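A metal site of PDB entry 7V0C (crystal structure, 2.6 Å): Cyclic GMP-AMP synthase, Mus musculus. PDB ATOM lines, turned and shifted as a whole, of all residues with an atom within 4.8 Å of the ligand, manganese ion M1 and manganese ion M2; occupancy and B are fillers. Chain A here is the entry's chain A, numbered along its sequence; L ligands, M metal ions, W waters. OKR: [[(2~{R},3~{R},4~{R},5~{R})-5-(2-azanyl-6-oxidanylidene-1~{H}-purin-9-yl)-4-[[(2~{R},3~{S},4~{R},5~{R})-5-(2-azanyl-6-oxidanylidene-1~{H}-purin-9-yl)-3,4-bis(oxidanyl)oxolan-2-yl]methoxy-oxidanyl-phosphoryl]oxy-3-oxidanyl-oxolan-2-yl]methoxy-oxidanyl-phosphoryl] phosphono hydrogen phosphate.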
ATOM      1  N   GLY A  55       1.839  26.188  20.720  1.00  0.00           N
ATOM      2  CA  GLY A  55       1.477  25.467  21.932  1.00  0.00           C
ATOM      3  C   GLY A  55       0.509  26.193  22.812  1.00  0.00           C
ATOM      4  O   GLY A  55      -0.025  27.246  22.448  1.00  0.00           O
ATOM      5  N   SER A  56       0.291  25.628  24.005  1.00  0.00           N
ATOM      6  CA  SER A  56      -0.847  25.970  24.848  1.00  0.00           C
ATOM      7  C   SER A  56      -0.864  27.423  25.277  1.00  0.00           C
ATOM      8  O   SER A  56      -1.906  28.057  25.290  1.00  0.00           O
ATOM      9  CB  SER A  56      -0.929  25.019  26.059  1.00  0.00           C
ATOM     10  OG  SER A  56       0.266  25.020  26.801  1.00  0.00           O
ATOM     11  N   GLU A  59      -2.024  29.548  22.508  1.00  0.00           N
ATOM     12  CA  GLU A  59      -3.397  29.177  22.191  1.00  0.00           C
ATOM     13  C   GLU A  59      -4.370  29.585  23.327  1.00  0.00           C
ATOM     14  O   GLU A  59      -5.584  29.479  23.174  1.00  0.00           O
ATOM     15  CB  GLU A  59      -3.477  27.679  21.932  1.00  0.00           C
ATOM     16  CG  GLU A  59      -2.695  27.193  20.710  1.00  0.00           C
ATOM     17  CD  GLU A  59      -2.508  25.676  20.673  1.00  0.00           C
ATOM     18  OE1 GLU A  59      -2.659  25.007  21.723  1.00  0.00           O
ATOM     19  OE2 GLU A  59      -2.194  25.128  19.582  1.00  0.00           O
ATOM     20  N   LYS A  62      -3.124  27.154  28.273  1.00  0.00           N
ATOM     21  CA  LYS A  62      -2.141  26.782  29.270  1.00  0.00           C
ATOM     22  C   LYS A  62      -2.824  26.877  30.612  1.00  0.00           C
ATOM     23  O   LYS A  62      -3.455  27.875  30.906  1.00  0.00           O
ATOM     24  CB  LYS A  62      -0.930  27.726  29.242  1.00  0.00           C
ATOM     25  CG  LYS A  62       0.183  27.340  30.215  1.00  0.00           C
ATOM     26  CD  LYS A  62       0.996  26.153  29.712  1.00  0.00           C
ATOM     27  CE  LYS A  62       2.069  25.780  30.735  1.00  0.00           C
ATOM     28  NZ  LYS A  62       1.520  25.173  31.969  1.00  0.00           N
ATOM     29  N   GLU A  68       5.666  26.641  30.893  1.00  0.00           N
ATOM     30  CA  GLU A  68       6.107  25.861  29.756  1.00  0.00           C
ATOM     31  C   GLU A  68       5.664  26.570  28.473  1.00  0.00           C
ATOM     32  O   GLU A  68       4.484  26.798  28.260  1.00  0.00           O
ATOM     33  CB  GLU A  68       5.579  24.415  29.855  1.00  0.00           C
ATOM     34  CG  GLU A  68       6.391  23.364  29.099  1.00  0.00           C
ATOM     35  CD  GLU A  68       6.001  23.262  27.616  1.00  0.00           C
ATOM     36  OE1 GLU A  68       5.199  24.101  27.168  1.00  0.00           O
ATOM     37  OE2 GLU A  68       6.492  22.353  26.885  1.00  0.00           O
ATOM     38  N   ASP A  70       6.426  27.026  24.090  1.00  0.00           N
ATOM     39  CA  ASP A  70       6.916  26.332  22.894  1.00  0.00           C
ATOM     40  C   ASP A  70       7.139  27.337  21.768  1.00  0.00           C
ATOM     41  O   ASP A  70       6.252  28.130  21.462  1.00  0.00           O
ATOM     42  CB  ASP A  70       5.948  25.226  22.470  1.00  0.00           C
ATOM     43  CG  ASP A  70       5.570  24.329  23.636  1.00  0.00           C
ATOM     44  OD1 ASP A  70       6.429  23.535  24.095  1.00  0.00           O
ATOM     45  OD2 ASP A  70       4.403  24.425  24.096  1.00  0.00           O
ATOM     46  N   LYS A 145      16.612  14.555  25.720  1.00  0.00           N
ATOM     47  CA  LYS A 145      15.735  13.413  25.767  1.00  0.00           C
ATOM     48  C   LYS A 145      15.651  12.833  24.365  1.00  0.00           C
ATOM     49  O   LYS A 145      15.384  13.563  23.422  1.00  0.00           O
ATOM     50  CB  LYS A 145      14.339  13.816  26.223  1.00  0.00           C
ATOM     51  CG  LYS A 145      14.317  14.310  27.655  1.00  0.00           C
ATOM     52  CD  LYS A 145      12.894  14.270  28.206  1.00  0.00           C
ATOM     53  CE  LYS A 145      12.717  15.169  29.422  1.00  0.00           C
ATOM     54  NZ  LYS A 145      13.885  15.173  30.350  1.00  0.00           N
ATOM     55  N   GLY A 147      13.925  10.951  21.172  1.00  0.00           N
ATOM     56  CA  GLY A 147      12.589  11.086  20.640  1.00  0.00           C
ATOM     57  C   GLY A 147      12.002  12.458  20.849  1.00  0.00           C
ATOM     58  O   GLY A 147      10.789  12.598  20.788  1.00  0.00           O
ATOM     59  N   ASP A 164      10.742  24.968  25.145  1.00  0.00           N
ATOM     60  CA  ASP A 164      11.139  24.083  24.064  1.00  0.00           C
ATOM     61  C   ASP A 164      11.380  24.915  22.812  1.00  0.00           C
ATOM     62  O   ASP A 164      10.460  25.547  22.293  1.00  0.00           O
ATOM     63  CB  ASP A 164      10.044  23.042  23.797  1.00  0.00           C
ATOM     64  CG  ASP A 164       9.852  22.073  24.945  1.00  0.00           C
ATOM     65  OD1 ASP A 164      10.793  21.828  25.748  1.00  0.00           O
ATOM     66  OD2 ASP A 164       8.741  21.522  25.039  1.00  0.00           O
ATOM     67  N   ARG A 221       9.486  14.436  11.116  1.00  0.00           N
ATOM     68  CA  ARG A 221       8.027  14.285  11.404  1.00  0.00           C
ATOM     69  C   ARG A 221       7.307  15.583  11.034  1.00  0.00           C
ATOM     70  O   ARG A 221       7.868  16.671  11.304  1.00  0.00           O
ATOM     71  CB  ARG A 221       7.797  13.940  12.887  1.00  0.00           C
ATOM     72  CG  ARG A 221       6.434  13.318  13.193  1.00  0.00           C
ATOM     73  CD  ARG A 221       5.970  13.625  14.607  1.00  0.00           C
ATOM     74  NE  ARG A 221       5.588  15.023  14.731  1.00  0.00           N
ATOM     75  CZ  ARG A 221       5.713  15.791  15.832  1.00  0.00           C
ATOM     76  NH1 ARG A 221       6.239  15.309  16.952  1.00  0.00           N
ATOM     77  NH2 ARG A 221       5.327  17.059  15.787  1.00  0.00           N
ATOM     78  N   LYS A 259      -7.152  18.406  29.806  1.00  0.00           N
ATOM     79  CA  LYS A 259      -5.708  18.577  29.994  1.00  0.00           C
ATOM     80  C   LYS A 259      -5.275  18.422  31.455  1.00  0.00           C
ATOM     81  O   LYS A 259      -4.261  17.770  31.747  1.00  0.00           O
ATOM     82  CB  LYS A 259      -5.282  19.953  29.532  1.00  0.00           C
ATOM     83  CG  LYS A 259      -5.125  20.092  28.035  1.00  0.00           C
ATOM     84  CD  LYS A 259      -4.955  21.555  27.655  1.00  0.00           C
ATOM     85  CE  LYS A 259      -3.626  22.158  28.080  1.00  0.00           C
ATOM     86  NZ  LYS A 259      -2.479  21.747  27.229  1.00  0.00           N
ATOM     87  N   GLU A 263      -2.753  15.705  33.227  1.00  0.00           N
ATOM     88  CA  GLU A 263      -1.605  16.177  34.016  1.00  0.00           C
ATOM     89  C   GLU A 263      -1.607  15.638  35.456  1.00  0.00           C
ATOM     90  O   GLU A 263      -0.589  15.143  35.940  1.00  0.00           O
ATOM     91  CB  GLU A 263      -1.540  17.715  34.077  1.00  0.00           C
ATOM     92  CG  GLU A 263      -0.980  18.388  32.842  1.00  0.00           C
ATOM     93  CD  GLU A 263      -0.794  19.888  33.001  1.00  0.00           C
ATOM     94  OE1 GLU A 263      -0.536  20.348  34.148  1.00  0.00           O
ATOM     95  OE2 GLU A 263      -0.883  20.608  31.959  1.00  0.00           O
ATOM     96  N   LYS A 266      -0.973  11.984  35.432  1.00  0.00           N
ATOM     97  CA  LYS A 266       0.369  11.726  34.964  1.00  0.00           C
ATOM     98  C   LYS A 266       1.429  11.982  36.029  1.00  0.00           C
ATOM     99  O   LYS A 266       2.426  11.258  36.106  1.00  0.00           O
ATOM    100  CB  LYS A 266       0.672  12.538  33.684  1.00  0.00           C
ATOM    101  CG  LYS A 266       0.335  11.777  32.401  1.00  0.00           C
ATOM    102  CD  LYS A 266       0.552  12.595  31.136  1.00  0.00           C
ATOM    103  CE  LYS A 266       2.034  12.897  30.858  1.00  0.00           C
ATOM    104  NZ  LYS A 266       2.836  11.671  30.685  1.00  0.00           N
ATOM    105  N   PHE A 275       1.353   8.604  27.559  1.00  0.00           N
ATOM    106  CA  PHE A 275       0.315   9.577  27.253  1.00  0.00           C
ATOM    107  C   PHE A 275       0.802  11.016  27.378  1.00  0.00           C
ATOM    108  O   PHE A 275       1.748  11.300  28.101  1.00  0.00           O
ATOM    109  CB  PHE A 275      -0.896   9.356  28.149  1.00  0.00           C
ATOM    110  CG  PHE A 275      -1.511   8.007  27.975  1.00  0.00           C
ATOM    111  CD1 PHE A 275      -2.298   7.725  26.868  1.00  0.00           C
ATOM    112  CD2 PHE A 275      -1.294   7.013  28.914  1.00  0.00           C
ATOM    113  CE1 PHE A 275      -2.855   6.475  26.696  1.00  0.00           C
ATOM    114  CE2 PHE A 275      -1.857   5.751  28.744  1.00  0.00           C
ATOM    115  CZ  PHE A 275      -2.640   5.491  27.637  1.00  0.00           C
ATOM    116  N   CYS A 276       0.136  11.927  26.658  1.00  0.00           N
ATOM    117  CA  CYS A 276       0.540  13.326  26.577  1.00  0.00           C
ATOM    118  C   CYS A 276      -0.649  14.212  26.243  1.00  0.00           C
ATOM    119  O   CYS A 276      -1.704  13.729  25.838  1.00  0.00           O
ATOM    120  CB  CYS A 276       1.632  13.493  25.511  1.00  0.00           C
ATOM    121  SG  CYS A 276       1.092  13.177  23.818  1.00  0.00           S
ATOM    122  N   SER A 277      -0.482  15.529  26.400  1.00  0.00           N
ATOM    123  CA  SER A 277      -1.553  16.459  26.170  1.00  0.00           C
ATOM    124  C   SER A 277      -1.995  16.466  24.704  1.00  0.00           C
ATOM    125  O   SER A 277      -3.147  16.801  24.399  1.00  0.00           O
ATOM    126  CB  SER A 277      -1.169  17.880  26.611  1.00  0.00           C
ATOM    127  OG  SER A 277      -0.046  18.350  25.897  1.00  0.00           O
ATOM    128  N   TYR A 278      -1.083  16.108  23.793  1.00  0.00           N
ATOM    129  CA  TYR A 278      -1.378  16.099  22.340  1.00  0.00           C
ATOM    130  C   TYR A 278      -2.486  15.082  22.036  1.00  0.00           C
ATOM    131  O   TYR A 278      -3.233  15.282  21.060  1.00  0.00           O
ATOM    132  CB  TYR A 278      -0.143  15.840  21.471  1.00  0.00           C
ATOM    133  CG  TYR A 278      -0.424  16.178  20.032  1.00  0.00           C
ATOM    134  CD1 TYR A 278      -0.546  17.510  19.660  1.00  0.00           C
ATOM    135  CD2 TYR A 278      -0.661  15.210  19.075  1.00  0.00           C
ATOM    136  CE1 TYR A 278      -0.859  17.869  18.355  1.00  0.00           C
ATOM    137  CE2 TYR A 278      -0.969  15.550  17.767  1.00  0.00           C
ATOM    138  CZ  TYR A 278      -1.073  16.883  17.410  1.00  0.00           C
ATOM    139  OH  TYR A 278      -1.381  17.252  16.125  1.00  0.00           O
ATOM    140  N   LYS A 281      -5.638  16.907  22.866  1.00  0.00           N
ATOM    141  CA  LYS A 281      -5.852  17.962  21.875  1.00  0.00           C
ATOM    142  C   LYS A 281      -6.434  17.388  20.588  1.00  0.00           C
ATOM    143  O   LYS A 281      -7.366  17.944  20.005  1.00  0.00           O
ATOM    144  CB  LYS A 281      -4.520  18.676  21.598  1.00  0.00           C
ATOM    145  CG  LYS A 281      -4.641  20.035  20.944  1.00  0.00           C
ATOM    146  CD  LYS A 281      -3.269  20.502  20.450  1.00  0.00           C
ATOM    147  CE  LYS A 281      -3.272  22.001  20.200  1.00  0.00           C
ATOM    148  NZ  LYS A 281      -2.075  22.463  19.411  1.00  0.00           N
ATOM    149  N   HIS A 324      -4.538  10.793  14.129  1.00  0.00           N
ATOM    150  CA  HIS A 324      -4.015  12.152  13.973  1.00  0.00           C
ATOM    151  C   HIS A 324      -5.021  12.930  13.141  1.00  0.00           C
ATOM    152  O   HIS A 324      -5.574  12.411  12.192  1.00  0.00           O
ATOM    153  CB  HIS A 324      -2.656  12.097  13.270  1.00  0.00           C
ATOM    154  CG  HIS A 324      -1.840  13.334  13.428  1.00  0.00           C
ATOM    155  ND1 HIS A 324      -2.191  14.543  12.863  1.00  0.00           N
ATOM    156  CD2 HIS A 324      -0.658  13.539  14.056  1.00  0.00           C
ATOM    157  CE1 HIS A 324      -1.266  15.441  13.151  1.00  0.00           C
ATOM    158  NE2 HIS A 324      -0.327  14.864  13.872  1.00  0.00           N
HETATM  159  N1  OKR L   1       4.481  20.103  27.985  1.00  0.00           N
HETATM  160  C1  OKR L   1       4.253  18.782  28.006  1.00  0.00           C
HETATM  161  N2  OKR L   1       5.274  17.923  27.924  1.00  0.00           N
HETATM  162  C2  OKR L   1       4.866  16.637  27.948  1.00  0.00           C
HETATM  163  C3  OKR L   1       3.582  16.143  28.054  1.00  0.00           C
HETATM  164  N3  OKR L   1       3.595  14.752  28.055  1.00  0.00           N
HETATM  165  C4  OKR L   1       4.867  14.435  27.951  1.00  0.00           C
HETATM  166  N4  OKR L   1       5.681  15.542  27.885  1.00  0.00           N
HETATM  167  C5  OKR L   1       7.148  15.582  27.773  1.00  0.00           C
HETATM  168  O1  OKR L   1       7.520  15.396  26.427  1.00  0.00           O
HETATM  169  C6  OKR L   1       8.805  14.719  26.363  1.00  0.00           C
HETATM  170  C7  OKR L   1       8.668  13.432  25.585  1.00  0.00           C
HETATM  171  O2  OKR L   1       8.044  13.696  24.298  1.00  0.00           O
HETATM  172  P1  OKR L   1       6.547  13.205  23.995  1.00  0.00           P
HETATM  173  O3  OKR L   1       6.444  12.850  22.537  1.00  0.00           O
HETATM  174  O4  OKR L   1       6.097  12.164  24.976  1.00  0.00           O
HETATM  175  O5  OKR L   1       5.756  14.577  24.313  1.00  0.00           O
HETATM  176  C8  OKR L   1       5.254  15.276  23.185  1.00  0.00           C
HETATM  177  C9  OKR L   1       5.050  16.743  23.552  1.00  0.00           C
HETATM  178  O6  OKR L   1       6.054  17.233  24.448  1.00  0.00           O
HETATM  179  C10 OKR L   1       3.686  16.694  24.241  1.00  0.00           C
HETATM  180  C11 OKR L   1       2.897  17.984  24.249  1.00  0.00           C
HETATM  181  O7  OKR L   1       3.770  19.069  24.647  1.00  0.00           O
HETATM  182  P2  OKR L   1       3.516  20.547  24.067  1.00  0.00           P
HETATM  183  O8  OKR L   1       3.826  20.543  22.606  1.00  0.00           O
HETATM  184  O9  OKR L   1       4.185  21.549  24.950  1.00  0.00           O
HETATM  185  O10 OKR L   1       1.946  20.713  24.290  1.00  0.00           O
HETATM  186  P3  OKR L   1       0.930  21.955  24.283  1.00  0.00           P
HETATM  187  O11 OKR L   1      -0.083  21.713  23.210  1.00  0.00           O
HETATM  188  O12 OKR L   1       1.693  23.235  24.292  1.00  0.00           O
HETATM  189  O13 OKR L   1       0.264  21.744  25.721  1.00  0.00           O
HETATM  190  P4  OKR L   1       0.922  21.717  27.202  1.00  0.00           P
HETATM  191  O14 OKR L   1       2.373  22.072  27.005  1.00  0.00           O
HETATM  192  O15 OKR L   1       0.739  20.314  27.711  1.00  0.00           O
HETATM  193  O16 OKR L   1       0.184  22.743  28.034  1.00  0.00           O
HETATM  194  O17 OKR L   1       2.948  15.693  23.497  1.00  0.00           O
HETATM  195  C12 OKR L   1       3.843  14.802  22.856  1.00  0.00           C
HETATM  196  N5  OKR L   1       3.531  14.774  21.431  1.00  0.00           N
HETATM  197  C13 OKR L   1       3.389  13.642  20.654  1.00  0.00           C
HETATM  198  N6  OKR L   1       3.108  13.906  19.406  1.00  0.00           N
HETATM  199  C14 OKR L   1       3.050  15.295  19.347  1.00  0.00           C
HETATM  200  C15 OKR L   1       2.780  16.164  18.260  1.00  0.00           C
HETATM  201  O18 OKR L   1       2.531  15.847  17.085  1.00  0.00           O
HETATM  202  N7  OKR L   1       2.828  17.505  18.644  1.00  0.00           N
HETATM  203  C16 OKR L   1       3.086  17.953  19.920  1.00  0.00           C
HETATM  204  N8  OKR L   1       3.080  19.283  20.108  1.00  0.00           N
HETATM  205  N9  OKR L   1       3.337  17.142  20.953  1.00  0.00           N
HETATM  206  C17 OKR L   1       3.309  15.843  20.596  1.00  0.00           C
HETATM  207  C18 OKR L   1       9.241  14.563  27.833  1.00  0.00           C
HETATM  208  O19 OKR L   1       9.999  15.674  28.271  1.00  0.00           O
HETATM  209  C19 OKR L   1       7.891  14.504  28.548  1.00  0.00           C
HETATM  210  O20 OKR L   1       8.011  14.782  29.928  1.00  0.00           O
HETATM  211  C20 OKR L   1       2.498  17.049  28.133  1.00  0.00           C
HETATM  212  O21 OKR L   1       1.290  16.805  28.243  1.00  0.00           O
HETATM  213  N10 OKR L   1       2.947  18.378  28.105  1.00  0.00           N
HETATM  214 MN    MN M   1       6.628  21.540  24.973  1.00  0.00          MN
HETATM  215 MN    MN M   2       3.509  23.391  25.824  1.00  0.00          MN
HETATM  216  O   HOH W   1      -0.638  23.318  30.399  1.00  0.00           O
HETATM  217  O   HOH W   2       2.858  25.338  26.431  1.00  0.00           O
HETATM  218  O   HOH W   3      -1.139  19.151  23.318  1.00  0.00           O
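Ser 56 touches manganese ion M2 (OG to MN, 3.8 Å).
Along chain A the residues within 4 Å of manganese ion M2 span positions 56 to 70.
The nearest printed residue that does not touch manganese ion M2 is Gly 55 (4.9 Å).
Within 4 Å of manganese ion M1: Glu 68, Asp 70 and Asp 164.
The nearest printed residue that does not touch manganese ion M1 is Gly 55 (7.2 Å).
O of Ser 56 is in hydrogen-bond range of N of Lys 62 (3.3 Å).
SG of Cys 276 lies close to N of Tyr 278.
NE2 of His 324 sits at hydrogen-bond distance from OH of Tyr 278 (3.4 Å).
The side-chain amino group of Lys 266 is in hydrogen-bond range of the backbone carbonyl oxygen of Phe 275, at 2.8 Å.
Residues that only touch the ligand: Gly 55 (3.3 Å), Lys 62 (3.9 Å), Lys 145 (3.0 Å), Lys 266 (3.7 Å), Phe 275 (3.9 Å) and Tyr 278 (3.5 Å).
Hydrophobic or aromatic side chains that line the ligand: Tyr 278.
13 residues have an atom within 4 Å of the ligand: Gly 55, Ser 56, Lys 62, Glu 68, Asp 70, Lys 145, Arg 221, Lys 259, Lys 266, Phe 275, Cys 276, Ser 277 and Tyr 278.
The nearest printed residue that does not touch the ligand is Lys 281 (4.4 Å).
The backbone NH (N) of Ser 56 sits close to an oxygen (O12) of the ligand (2.8 Å).
An oxygen (O16) of the ligand sits at hydrogen-bond distance from the side-chain hydroxyl (OG) of Ser 56, at 2.6 Å.
An oxygen (O21) of the ligand is in hydrogen-bond range of the backbone NH (N) of Ser 277, 2.9 Å away.
The side-chain hydroxyl of Ser 277 is in hydrogen-bond range of an oxygen (O15) of the ligand.
The side-chain amino group (NZ) of Lys 259 is in salt-bridge range of an oxygen (O16) of the ligand (3.0 Å).
The side-chain sulfur of Cys 276 is in hydrogen-bond range of an oxygen (O17) of the ligand (3.1 Å).
An oxygen (O18) of the ligand is in hydrogen-bond range of the guanidinium group of Arg 221 (3.3 Å).
Water W2 lies within hydrogen-bond range of OG of Ser 56 (2.6 Å) and O of Glu 68 (2.8 Å).
Water W1 lies within hydrogen-bond range of O16 of the ligand (2.6 Å), OE2 of Glu 263 (3.1 Å) and NZ of Lys 62 (3.3 Å).
Water W3 lies within hydrogen-bond range of an oxygen (O11) of the ligand (2.8 Å), the side-chain hydroxyl (OG) of Ser 277 (2.9 Å) and the backbone NH (N) of Tyr 278 (3.1 Å).
Manganese ion M1 is bound by OE2 of Glu 68 (2.1 Å), OD2 of Asp 164 (2.1 Å), OD1 of Asp 70 (2.2 Å) and O9 of the ligand (2.4 Å).
Manganese ion M1 has four donor atoms within binding distance.
Manganese ion M2 is bound by an oxygen (O14) of the ligand (2.1 Å), water W2 (2.1 Å), an oxygen (O9) of the ligand (2.1 Å), the side-chain carboxylate (OD2) of Asp 70 (2.2 Å), the side-chain carboxylate (OE1) of Glu 68 (2.3 Å) and an oxygen (O12) of the ligand (2.4 Å).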
